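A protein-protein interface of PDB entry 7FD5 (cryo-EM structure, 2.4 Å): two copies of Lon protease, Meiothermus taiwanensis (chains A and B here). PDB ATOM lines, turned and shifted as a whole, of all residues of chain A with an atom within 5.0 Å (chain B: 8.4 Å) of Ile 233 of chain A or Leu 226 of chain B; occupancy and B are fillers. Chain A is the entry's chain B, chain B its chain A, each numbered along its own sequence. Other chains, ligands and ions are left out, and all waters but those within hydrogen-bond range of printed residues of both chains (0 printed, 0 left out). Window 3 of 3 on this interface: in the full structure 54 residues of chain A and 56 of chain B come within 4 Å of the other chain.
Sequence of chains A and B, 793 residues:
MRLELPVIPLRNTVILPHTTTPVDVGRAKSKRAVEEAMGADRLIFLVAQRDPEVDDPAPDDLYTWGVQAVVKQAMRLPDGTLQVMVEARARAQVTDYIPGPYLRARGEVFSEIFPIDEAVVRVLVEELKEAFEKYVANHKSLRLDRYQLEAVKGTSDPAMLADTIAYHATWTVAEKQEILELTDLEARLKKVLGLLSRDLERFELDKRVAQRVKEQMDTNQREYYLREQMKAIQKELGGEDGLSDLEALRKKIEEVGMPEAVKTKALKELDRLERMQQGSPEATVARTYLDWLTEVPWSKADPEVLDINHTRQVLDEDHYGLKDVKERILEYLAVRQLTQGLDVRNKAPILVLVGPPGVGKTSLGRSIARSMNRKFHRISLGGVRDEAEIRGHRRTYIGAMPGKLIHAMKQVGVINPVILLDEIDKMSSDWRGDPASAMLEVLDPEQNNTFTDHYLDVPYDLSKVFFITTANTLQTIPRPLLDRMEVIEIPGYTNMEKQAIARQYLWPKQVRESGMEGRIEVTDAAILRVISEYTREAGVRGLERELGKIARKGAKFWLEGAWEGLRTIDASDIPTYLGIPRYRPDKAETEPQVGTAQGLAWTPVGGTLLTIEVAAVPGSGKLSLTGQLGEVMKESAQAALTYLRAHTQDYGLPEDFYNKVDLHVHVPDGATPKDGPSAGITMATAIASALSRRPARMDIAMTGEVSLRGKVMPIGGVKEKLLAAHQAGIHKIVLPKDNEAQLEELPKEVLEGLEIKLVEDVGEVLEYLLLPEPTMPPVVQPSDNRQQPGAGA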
ATOM      1  N   GLN A 229     -24.193  21.452  27.062  1.00  0.00           N
ATOM      2  CA  GLN A 229     -23.494  20.527  26.176  1.00  0.00           C
ATOM      3  C   GLN A 229     -22.087  21.023  25.898  1.00  0.00           C
ATOM      4  O   GLN A 229     -21.128  20.238  25.911  1.00  0.00           O
ATOM      5  CB  GLN A 229     -24.270  20.343  24.873  1.00  0.00           C
ATOM      6  CG  GLN A 229     -25.609  19.602  24.998  1.00  0.00           C
ATOM      7  CD  GLN A 229     -25.474  18.104  25.205  1.00  0.00           C
ATOM      8  OE1 GLN A 229     -24.661  17.447  24.561  1.00  0.00           O
ATOM      9  NE2 GLN A 229     -26.273  17.559  26.112  1.00  0.00           N
ATOM     10  N   MET A 230     -21.947  22.338  25.729  1.00  0.00           N
ATOM     11  CA  MET A 230     -20.638  22.945  25.599  1.00  0.00           C
ATOM     12  C   MET A 230     -19.801  22.748  26.852  1.00  0.00           C
ATOM     13  O   MET A 230     -18.583  22.582  26.758  1.00  0.00           O
ATOM     14  CB  MET A 230     -20.812  24.419  25.260  1.00  0.00           C
ATOM     15  CG  MET A 230     -19.521  25.168  25.115  1.00  0.00           C
ATOM     16  SD  MET A 230     -19.672  26.813  24.420  1.00  0.00           S
ATOM     17  CE  MET A 230     -19.770  26.398  22.680  1.00  0.00           C
ATOM     18  N   LYS A 231     -20.437  22.687  28.018  1.00  0.00           N
ATOM     19  CA  LYS A 231     -19.679  22.481  29.242  1.00  0.00           C
ATOM     20  C   LYS A 231     -19.163  21.059  29.336  1.00  0.00           C
ATOM     21  O   LYS A 231     -18.017  20.846  29.729  1.00  0.00           O
ATOM     22  CB  LYS A 231     -20.518  22.833  30.470  1.00  0.00           C
ATOM     23  CG  LYS A 231     -19.758  22.605  31.777  1.00  0.00           C
ATOM     24  CD  LYS A 231     -18.519  23.493  31.883  1.00  0.00           C
ATOM     25  CE  LYS A 231     -17.607  23.022  32.997  1.00  0.00           C
ATOM     26  NZ  LYS A 231     -18.264  23.059  34.318  1.00  0.00           N
ATOM     27  N   ALA A 232     -19.984  20.083  28.955  1.00  0.00           N
ATOM     28  CA  ALA A 232     -19.515  18.695  28.939  1.00  0.00           C
ATOM     29  C   ALA A 232     -18.370  18.506  27.948  1.00  0.00           C
ATOM     30  O   ALA A 232     -17.371  17.835  28.246  1.00  0.00           O
ATOM     31  CB  ALA A 232     -20.670  17.749  28.602  1.00  0.00           C
ATOM     32  N   ILE A 233     -18.467  19.157  26.793  1.00  0.00           N
ATOM     33  CA  ILE A 233     -17.433  18.996  25.782  1.00  0.00           C
ATOM     34  C   ILE A 233     -16.142  19.699  26.201  1.00  0.00           C
ATOM     35  O   ILE A 233     -15.065  19.093  26.212  1.00  0.00           O
ATOM     36  CB  ILE A 233     -17.954  19.482  24.420  1.00  0.00           C
ATOM     37  CG1 ILE A 233     -19.141  18.627  23.994  1.00  0.00           C
ATOM     38  CG2 ILE A 233     -16.889  19.421  23.380  1.00  0.00           C
ATOM     39  CD1 ILE A 233     -18.849  17.156  23.973  1.00  0.00           C
ATOM     40  N   GLN A 234     -16.225  20.974  26.585  1.00  0.00           N
ATOM     41  CA  GLN A 234     -15.017  21.688  26.975  1.00  0.00           C
ATOM     42  C   GLN A 234     -14.475  21.190  28.317  1.00  0.00           C
ATOM     43  O   GLN A 234     -13.278  21.334  28.588  1.00  0.00           O
ATOM     44  CB  GLN A 234     -15.302  23.190  26.967  1.00  0.00           C
ATOM     45  CG  GLN A 234     -14.076  24.064  27.114  1.00  0.00           C
ATOM     46  CD  GLN A 234     -13.106  23.914  25.970  1.00  0.00           C
ATOM     47  OE1 GLN A 234     -13.504  23.908  24.816  1.00  0.00           O
ATOM     48  NE2 GLN A 234     -11.822  23.767  26.286  1.00  0.00           N
ATOM     49  N   LYS A 235     -15.317  20.558  29.132  1.00  0.00           N
ATOM     50  CA  LYS A 235     -14.851  19.687  30.195  1.00  0.00           C
ATOM     51  C   LYS A 235     -13.925  18.620  29.643  1.00  0.00           C
ATOM     52  O   LYS A 235     -12.786  18.487  30.095  1.00  0.00           O
ATOM     53  CB  LYS A 235     -16.060  19.077  30.915  1.00  0.00           C
ATOM     54  CG  LYS A 235     -15.753  17.956  31.889  1.00  0.00           C
ATOM     55  CD  LYS A 235     -16.186  16.611  31.299  1.00  0.00           C
ATOM     56  CE  LYS A 235     -15.783  15.419  32.155  1.00  0.00           C
ATOM     57  NZ  LYS A 235     -16.456  15.346  33.472  1.00  0.00           N
ATOM     58  N   GLU A 236     -14.367  17.899  28.599  1.00  0.00           N
ATOM     59  CA  GLU A 236     -13.468  16.896  28.020  1.00  0.00           C
ATOM     60  C   GLU A 236     -12.383  17.488  27.148  1.00  0.00           C
ATOM     61  O   GLU A 236     -11.660  16.733  26.508  1.00  0.00           O
ATOM     62  CB  GLU A 236     -14.239  15.853  27.230  1.00  0.00           C
ATOM     63  CG  GLU A 236     -14.961  14.855  28.125  1.00  0.00           C
ATOM     64  CD  GLU A 236     -15.756  13.813  27.352  1.00  0.00           C
ATOM     65  OE1 GLU A 236     -15.886  13.940  26.117  1.00  0.00           O
ATOM     66  OE2 GLU A 236     -16.250  12.860  27.987  1.00  0.00           O
ATOM     67  N   LEU A 237     -12.311  18.810  27.055  1.00  0.00           N
ATOM     68  CA  LEU A 237     -11.066  19.530  26.776  1.00  0.00           C
ATOM     69  C   LEU A 237     -10.520  20.359  27.937  1.00  0.00           C
ATOM     70  O   LEU A 237      -9.898  21.397  27.689  1.00  0.00           O
ATOM     71  CB  LEU A 237     -11.198  20.437  25.544  1.00  0.00           C
ATOM     72  CG  LEU A 237     -10.319  20.049  24.358  1.00  0.00           C
ATOM     73  CD1 LEU A 237      -8.891  20.467  24.677  1.00  0.00           C
ATOM     74  CD2 LEU A 237     -10.349  18.571  24.103  1.00  0.00           C
ATOM     75  N   THR B 219      -7.879   8.500  20.080  1.00  0.00           N
ATOM     76  CA  THR B 219      -7.971   9.663  20.957  1.00  0.00           C
ATOM     77  C   THR B 219      -7.833  10.982  20.196  1.00  0.00           C
ATOM     78  O   THR B 219      -8.601  11.926  20.437  1.00  0.00           O
ATOM     79  CB  THR B 219      -6.913   9.591  22.046  1.00  0.00           C
ATOM     80  OG1 THR B 219      -5.614   9.558  21.444  1.00  0.00           O
ATOM     81  CG2 THR B 219      -7.129   8.365  22.916  1.00  0.00           C
ATOM     82  N   ASN B 220      -6.866  11.083  19.284  1.00  0.00           N
ATOM     83  CA  ASN B 220      -6.716  12.386  18.626  1.00  0.00           C
ATOM     84  C   ASN B 220      -7.827  12.673  17.624  1.00  0.00           C
ATOM     85  O   ASN B 220      -8.212  13.842  17.452  1.00  0.00           O
ATOM     86  CB  ASN B 220      -5.352  12.551  17.970  1.00  0.00           C
ATOM     87  CG  ASN B 220      -4.328  13.157  18.909  1.00  0.00           C
ATOM     88  OD1 ASN B 220      -3.347  12.526  19.276  1.00  0.00           O
ATOM     89  ND2 ASN B 220      -4.557  14.404  19.293  1.00  0.00           N
ATOM     90  N   GLN B 221      -8.394  11.645  16.989  1.00  0.00           N
ATOM     91  CA  GLN B 221      -9.548  11.945  16.142  1.00  0.00           C
ATOM     92  C   GLN B 221     -10.739  12.365  16.994  1.00  0.00           C
ATOM     93  O   GLN B 221     -11.549  13.208  16.573  1.00  0.00           O
ATOM     94  CB  GLN B 221      -9.899  10.763  15.230  1.00  0.00           C
ATOM     95  CG  GLN B 221     -10.423   9.488  15.887  1.00  0.00           C
ATOM     96  CD  GLN B 221     -11.926   9.487  16.075  1.00  0.00           C
ATOM     97  OE1 GLN B 221     -12.658  10.074  15.286  1.00  0.00           O
ATOM     98  NE2 GLN B 221     -12.388   8.857  17.144  1.00  0.00           N
ATOM     99  N   ARG B 222     -10.827  11.827  18.220  1.00  0.00           N
ATOM    100  CA  ARG B 222     -11.880  12.245  19.135  1.00  0.00           C
ATOM    101  C   ARG B 222     -11.744  13.713  19.483  1.00  0.00           C
ATOM    102  O   ARG B 222     -12.739  14.447  19.499  1.00  0.00           O
ATOM    103  CB  ARG B 222     -11.834  11.408  20.409  1.00  0.00           C
ATOM    104  CG  ARG B 222     -12.968  11.683  21.353  1.00  0.00           C
ATOM    105  CD  ARG B 222     -14.239  11.075  20.826  1.00  0.00           C
ATOM    106  NE  ARG B 222     -15.380  11.320  21.700  1.00  0.00           N
ATOM    107  CZ  ARG B 222     -16.217  12.339  21.557  1.00  0.00           C
ATOM    108  NH1 ARG B 222     -16.054  13.196  20.566  1.00  0.00           N
ATOM    109  NH2 ARG B 222     -17.230  12.490  22.389  1.00  0.00           N
ATOM    110  N   GLU B 223     -10.520  14.160  19.743  1.00  0.00           N
ATOM    111  CA  GLU B 223     -10.345  15.545  20.168  1.00  0.00           C
ATOM    112  C   GLU B 223     -10.600  16.513  19.014  1.00  0.00           C
ATOM    113  O   GLU B 223     -11.155  17.607  19.221  1.00  0.00           O
ATOM    114  CB  GLU B 223      -8.957  15.737  20.780  1.00  0.00           C
ATOM    115  CG  GLU B 223      -8.764  14.918  22.067  1.00  0.00           C
ATOM    116  CD  GLU B 223      -7.402  15.092  22.724  1.00  0.00           C
ATOM    117  OE1 GLU B 223      -6.585  15.885  22.210  1.00  0.00           O
ATOM    118  OE2 GLU B 223      -7.140  14.400  23.735  1.00  0.00           O
ATOM    119  N   TYR B 224     -10.249  16.102  17.786  1.00  0.00           N
ATOM    120  CA  TYR B 224     -10.691  16.843  16.600  1.00  0.00           C
ATOM    121  C   TYR B 224     -12.207  16.971  16.527  1.00  0.00           C
ATOM    122  O   TYR B 224     -12.731  18.050  16.192  1.00  0.00           O
ATOM    123  CB  TYR B 224     -10.178  16.165  15.332  1.00  0.00           C
ATOM    124  CG  TYR B 224     -10.872  16.621  14.061  1.00  0.00           C
ATOM    125  CD1 TYR B 224     -10.661  17.889  13.544  1.00  0.00           C
ATOM    126  CD2 TYR B 224     -11.727  15.759  13.363  1.00  0.00           C
ATOM    127  CE1 TYR B 224     -11.295  18.294  12.376  1.00  0.00           C
ATOM    128  CE2 TYR B 224     -12.362  16.158  12.194  1.00  0.00           C
ATOM    129  CZ  TYR B 224     -12.146  17.426  11.707  1.00  0.00           C
ATOM    130  OH  TYR B 224     -12.774  17.831  10.551  1.00  0.00           O
ATOM    131  N   TYR B 225     -12.921  15.892  16.850  1.00  0.00           N
ATOM    132  CA  TYR B 225     -14.373  15.968  16.792  1.00  0.00           C
ATOM    133  C   TYR B 225     -14.929  16.923  17.835  1.00  0.00           C
ATOM    134  O   TYR B 225     -15.910  17.636  17.566  1.00  0.00           O
ATOM    135  CB  TYR B 225     -15.009  14.600  16.970  1.00  0.00           C
ATOM    136  CG  TYR B 225     -16.481  14.775  16.878  1.00  0.00           C
ATOM    137  CD1 TYR B 225     -17.046  15.137  15.681  1.00  0.00           C
ATOM    138  CD2 TYR B 225     -17.295  14.674  17.992  1.00  0.00           C
ATOM    139  CE1 TYR B 225     -18.380  15.353  15.574  1.00  0.00           C
ATOM    140  CE2 TYR B 225     -18.631  14.887  17.898  1.00  0.00           C
ATOM    141  CZ  TYR B 225     -19.177  15.225  16.682  1.00  0.00           C
ATOM    142  OH  TYR B 225     -20.532  15.436  16.572  1.00  0.00           O
ATOM    143  N   LEU B 226     -14.363  16.883  19.045  1.00  0.00           N
ATOM    144  CA  LEU B 226     -14.757  17.825  20.086  1.00  0.00           C
ATOM    145  C   LEU B 226     -14.661  19.242  19.592  1.00  0.00           C
ATOM    146  O   LEU B 226     -15.650  19.984  19.647  1.00  0.00           O
ATOM    147  CB  LEU B 226     -13.900  17.690  21.338  1.00  0.00           C
ATOM    148  CG  LEU B 226     -14.412  16.860  22.506  1.00  0.00           C
ATOM    149  CD1 LEU B 226     -14.266  15.390  22.316  1.00  0.00           C
ATOM    150  CD2 LEU B 226     -13.734  17.290  23.771  1.00  0.00           C
ATOM    151  N   ARG B 227     -13.514  19.599  19.018  1.00  0.00           N
ATOM    152  CA  ARG B 227     -13.308  20.992  18.643  1.00  0.00           C
ATOM    153  C   ARG B 227     -14.217  21.397  17.486  1.00  0.00           C
ATOM    154  O   ARG B 227     -14.664  22.548  17.418  1.00  0.00           O
ATOM    155  CB  ARG B 227     -11.836  21.241  18.317  1.00  0.00           C
ATOM    156  CG  ARG B 227     -10.893  20.918  19.481  1.00  0.00           C
ATOM    157  CD  ARG B 227     -11.194  21.799  20.668  1.00  0.00           C
ATOM    158  NE  ARG B 227     -10.982  23.199  20.325  1.00  0.00           N
ATOM    159  CZ  ARG B 227     -11.452  24.239  21.007  1.00  0.00           C
ATOM    160  NH1 ARG B 227     -11.192  25.458  20.580  1.00  0.00           N
ATOM    161  NH2 ARG B 227     -12.178  24.065  22.101  1.00  0.00           N
ATOM    162  N   GLU B 228     -14.602  20.445  16.629  1.00  0.00           N
ATOM    163  CA  GLU B 228     -15.484  20.854  15.536  1.00  0.00           C
ATOM    164  C   GLU B 228     -16.952  20.924  15.945  1.00  0.00           C
ATOM    165  O   GLU B 228     -17.708  21.744  15.397  1.00  0.00           O
ATOM    166  CB  GLU B 228     -15.290  19.950  14.335  1.00  0.00           C
ATOM    167  CG  GLU B 228     -14.005  20.261  13.597  1.00  0.00           C
ATOM    168  CD  GLU B 228     -14.049  21.613  12.900  1.00  0.00           C
ATOM    169  OE1 GLU B 228     -15.145  22.029  12.480  1.00  0.00           O
ATOM    170  OE2 GLU B 228     -12.991  22.254  12.751  1.00  0.00           O
ATOM    171  N   GLN B 229     -17.381  20.128  16.922  1.00  0.00           N
ATOM    172  CA  GLN B 229     -18.736  20.327  17.423  1.00  0.00           C
ATOM    173  C   GLN B 229     -18.820  21.626  18.211  1.00  0.00           C
ATOM    174  O   GLN B 229     -19.830  22.346  18.148  1.00  0.00           O
ATOM    175  CB  GLN B 229     -19.184  19.137  18.264  1.00  0.00           C
ATOM    176  CG  GLN B 229     -20.663  19.179  18.594  1.00  0.00           C
ATOM    177  CD  GLN B 229     -21.175  17.902  19.234  1.00  0.00           C
ATOM    178  OE1 GLN B 229     -20.417  16.972  19.474  1.00  0.00           O
ATOM    179  NE2 GLN B 229     -22.470  17.852  19.508  1.00  0.00           N
ATOM    180  N   MET B 230     -17.735  21.967  18.913  1.00  0.00           N
ATOM    181  CA  MET B 230     -17.639  23.271  19.555  1.00  0.00           C
ATOM    182  C   MET B 230     -17.717  24.389  18.542  1.00  0.00           C
ATOM    183  O   MET B 230     -18.368  25.406  18.793  1.00  0.00           O
ATOM    184  CB  MET B 230     -16.333  23.376  20.320  1.00  0.00           C
ATOM    185  CG  MET B 230     -16.271  22.529  21.550  1.00  0.00           C
ATOM    186  SD  MET B 230     -17.292  23.101  22.897  1.00  0.00           S
ATOM    187  CE  MET B 230     -16.330  24.524  23.353  1.00  0.00           C
ATOM    188  N   LYS B 231     -17.049  24.214  17.401  1.00  0.00           N
ATOM    189  CA  LYS B 231     -17.059  25.228  16.352  1.00  0.00           C
ATOM    190  C   LYS B 231     -18.462  25.431  15.797  1.00  0.00           C
ATOM    191  O   LYS B 231     -18.870  26.565  15.528  1.00  0.00           O
ATOM    192  CB  LYS B 231     -16.087  24.831  15.245  1.00  0.00           C
ATOM    193  CG  LYS B 231     -14.616  24.835  15.628  1.00  0.00           C
ATOM    194  CD  LYS B 231     -13.718  24.402  14.470  1.00  0.00           C
ATOM    195  CE  LYS B 231     -12.241  24.429  14.846  1.00  0.00           C
ATOM    196  NZ  LYS B 231     -11.369  23.991  13.741  1.00  0.00           N
ATOM    197  N   ALA B 232     -19.240  24.352  15.698  1.00  0.00           N
ATOM    198  CA  ALA B 232     -20.625  24.490  15.243  1.00  0.00           C
ATOM    199  C   ALA B 232     -21.495  25.225  16.266  1.00  0.00           C
ATOM    200  O   ALA B 232     -22.302  26.096  15.902  1.00  0.00           O
ATOM    201  CB  ALA B 232     -21.211  23.114  14.930  1.00  0.00           C
ATOM    202  N   ILE B 233     -21.329  24.911  17.553  1.00  0.00           N
ATOM    203  CA  ILE B 233     -22.143  25.581  18.566  1.00  0.00           C
ATOM    204  C   ILE B 233     -21.784  27.065  18.665  1.00  0.00           C
ATOM    205  O   ILE B 233     -22.666  27.933  18.756  1.00  0.00           O
ATOM    206  CB  ILE B 233     -21.996  24.874  19.920  1.00  0.00           C
ATOM    207  CG1 ILE B 233     -22.416  23.427  19.795  1.00  0.00           C
ATOM    208  CG2 ILE B 233     -22.910  25.495  20.946  1.00  0.00           C
ATOM    209  CD1 ILE B 233     -22.119  22.636  21.030  1.00  0.00           C
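The guanidinium group of Arg 227 of chain B is in hydrogen-bond range of the side-chain amide oxygen of Gln 234 of chain A (3.0 Å).
NE2 of Gln 234 of chain A sits at hydrogen-bond distance from O of Leu 237 of chain A, 3.4 Å away.
Among the printed residues, merely in contact across the chains: Met 230 of chain A with Met 230 of chain B, Met 230 of chain A with Ile 233 of chain B, Ile 233 of chain A with Leu 226 of chain B, Ile 233 of chain A with Met 230 of chain B, Gln 234 of chain A with Met 230 of chain B, Glu 236 of chain A with Leu 226 of chain B and Leu 237 of chain A with Leu 226 of chain B.
Ile 233 of chain A touches just these residues of chain B: Leu 226 and Met 230. Of the printed residues of chain B, Leu 237 of chain A touches Leu 226. Gln 221 of chain B touches none of the printed residues of chain A. Leu 226 of chain B touches just these residues of chain A: Ile 233, Glu 236 and Leu 237. Of the printed residues of chain A, Arg 227 of chain B touches Gln 234 (3.0 Å). Glu 228 of chain B touches none of the printed residues of chain A. Of the printed residues of chain A, Met 230 of chain B touches Met 230 (3.7 Å), Ile 233 (3.7 Å) and Gln 234 (3.2 Å). Printed residues of chain A within 4 Å of Ile 233 of chain B: Met 230. The nearest residue of chain B that does not touch Ile 233 of chain A is Gln 229 of chain B (4.8 Å). The nearest printed residue of chain A that does not touch Leu 226 of chain B is Gln 234 of chain A (5.3 Å). The nearest printed residue of chain A that does not touch Arg 227 of chain B is Leu 237 of chain A (4.2 Å).
Printed residues of chain B that touch a printed residue of chain A: Leu 226, Arg 227, Met 230 and Ile 233. Among the printed residues, 8 pairs touch across the chains. Among the printed residues, no Asp or Glu carboxylate lies within 4 Å of a Lys or Arg side-chain nitrogen of the other chain.
Met 230 of chain A touches its own counterpart, Met 230 of chain B. Met 230 of chain A touches Ile 233 of chain B, and with the chains exchanged Ile 233 of chain A touches Met 230 of chain B. 5 positions are printed for both chains. Of the 8 pairs that touch across the chains among the printed residues, 3 have their exchanged pair printed and touching as well.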
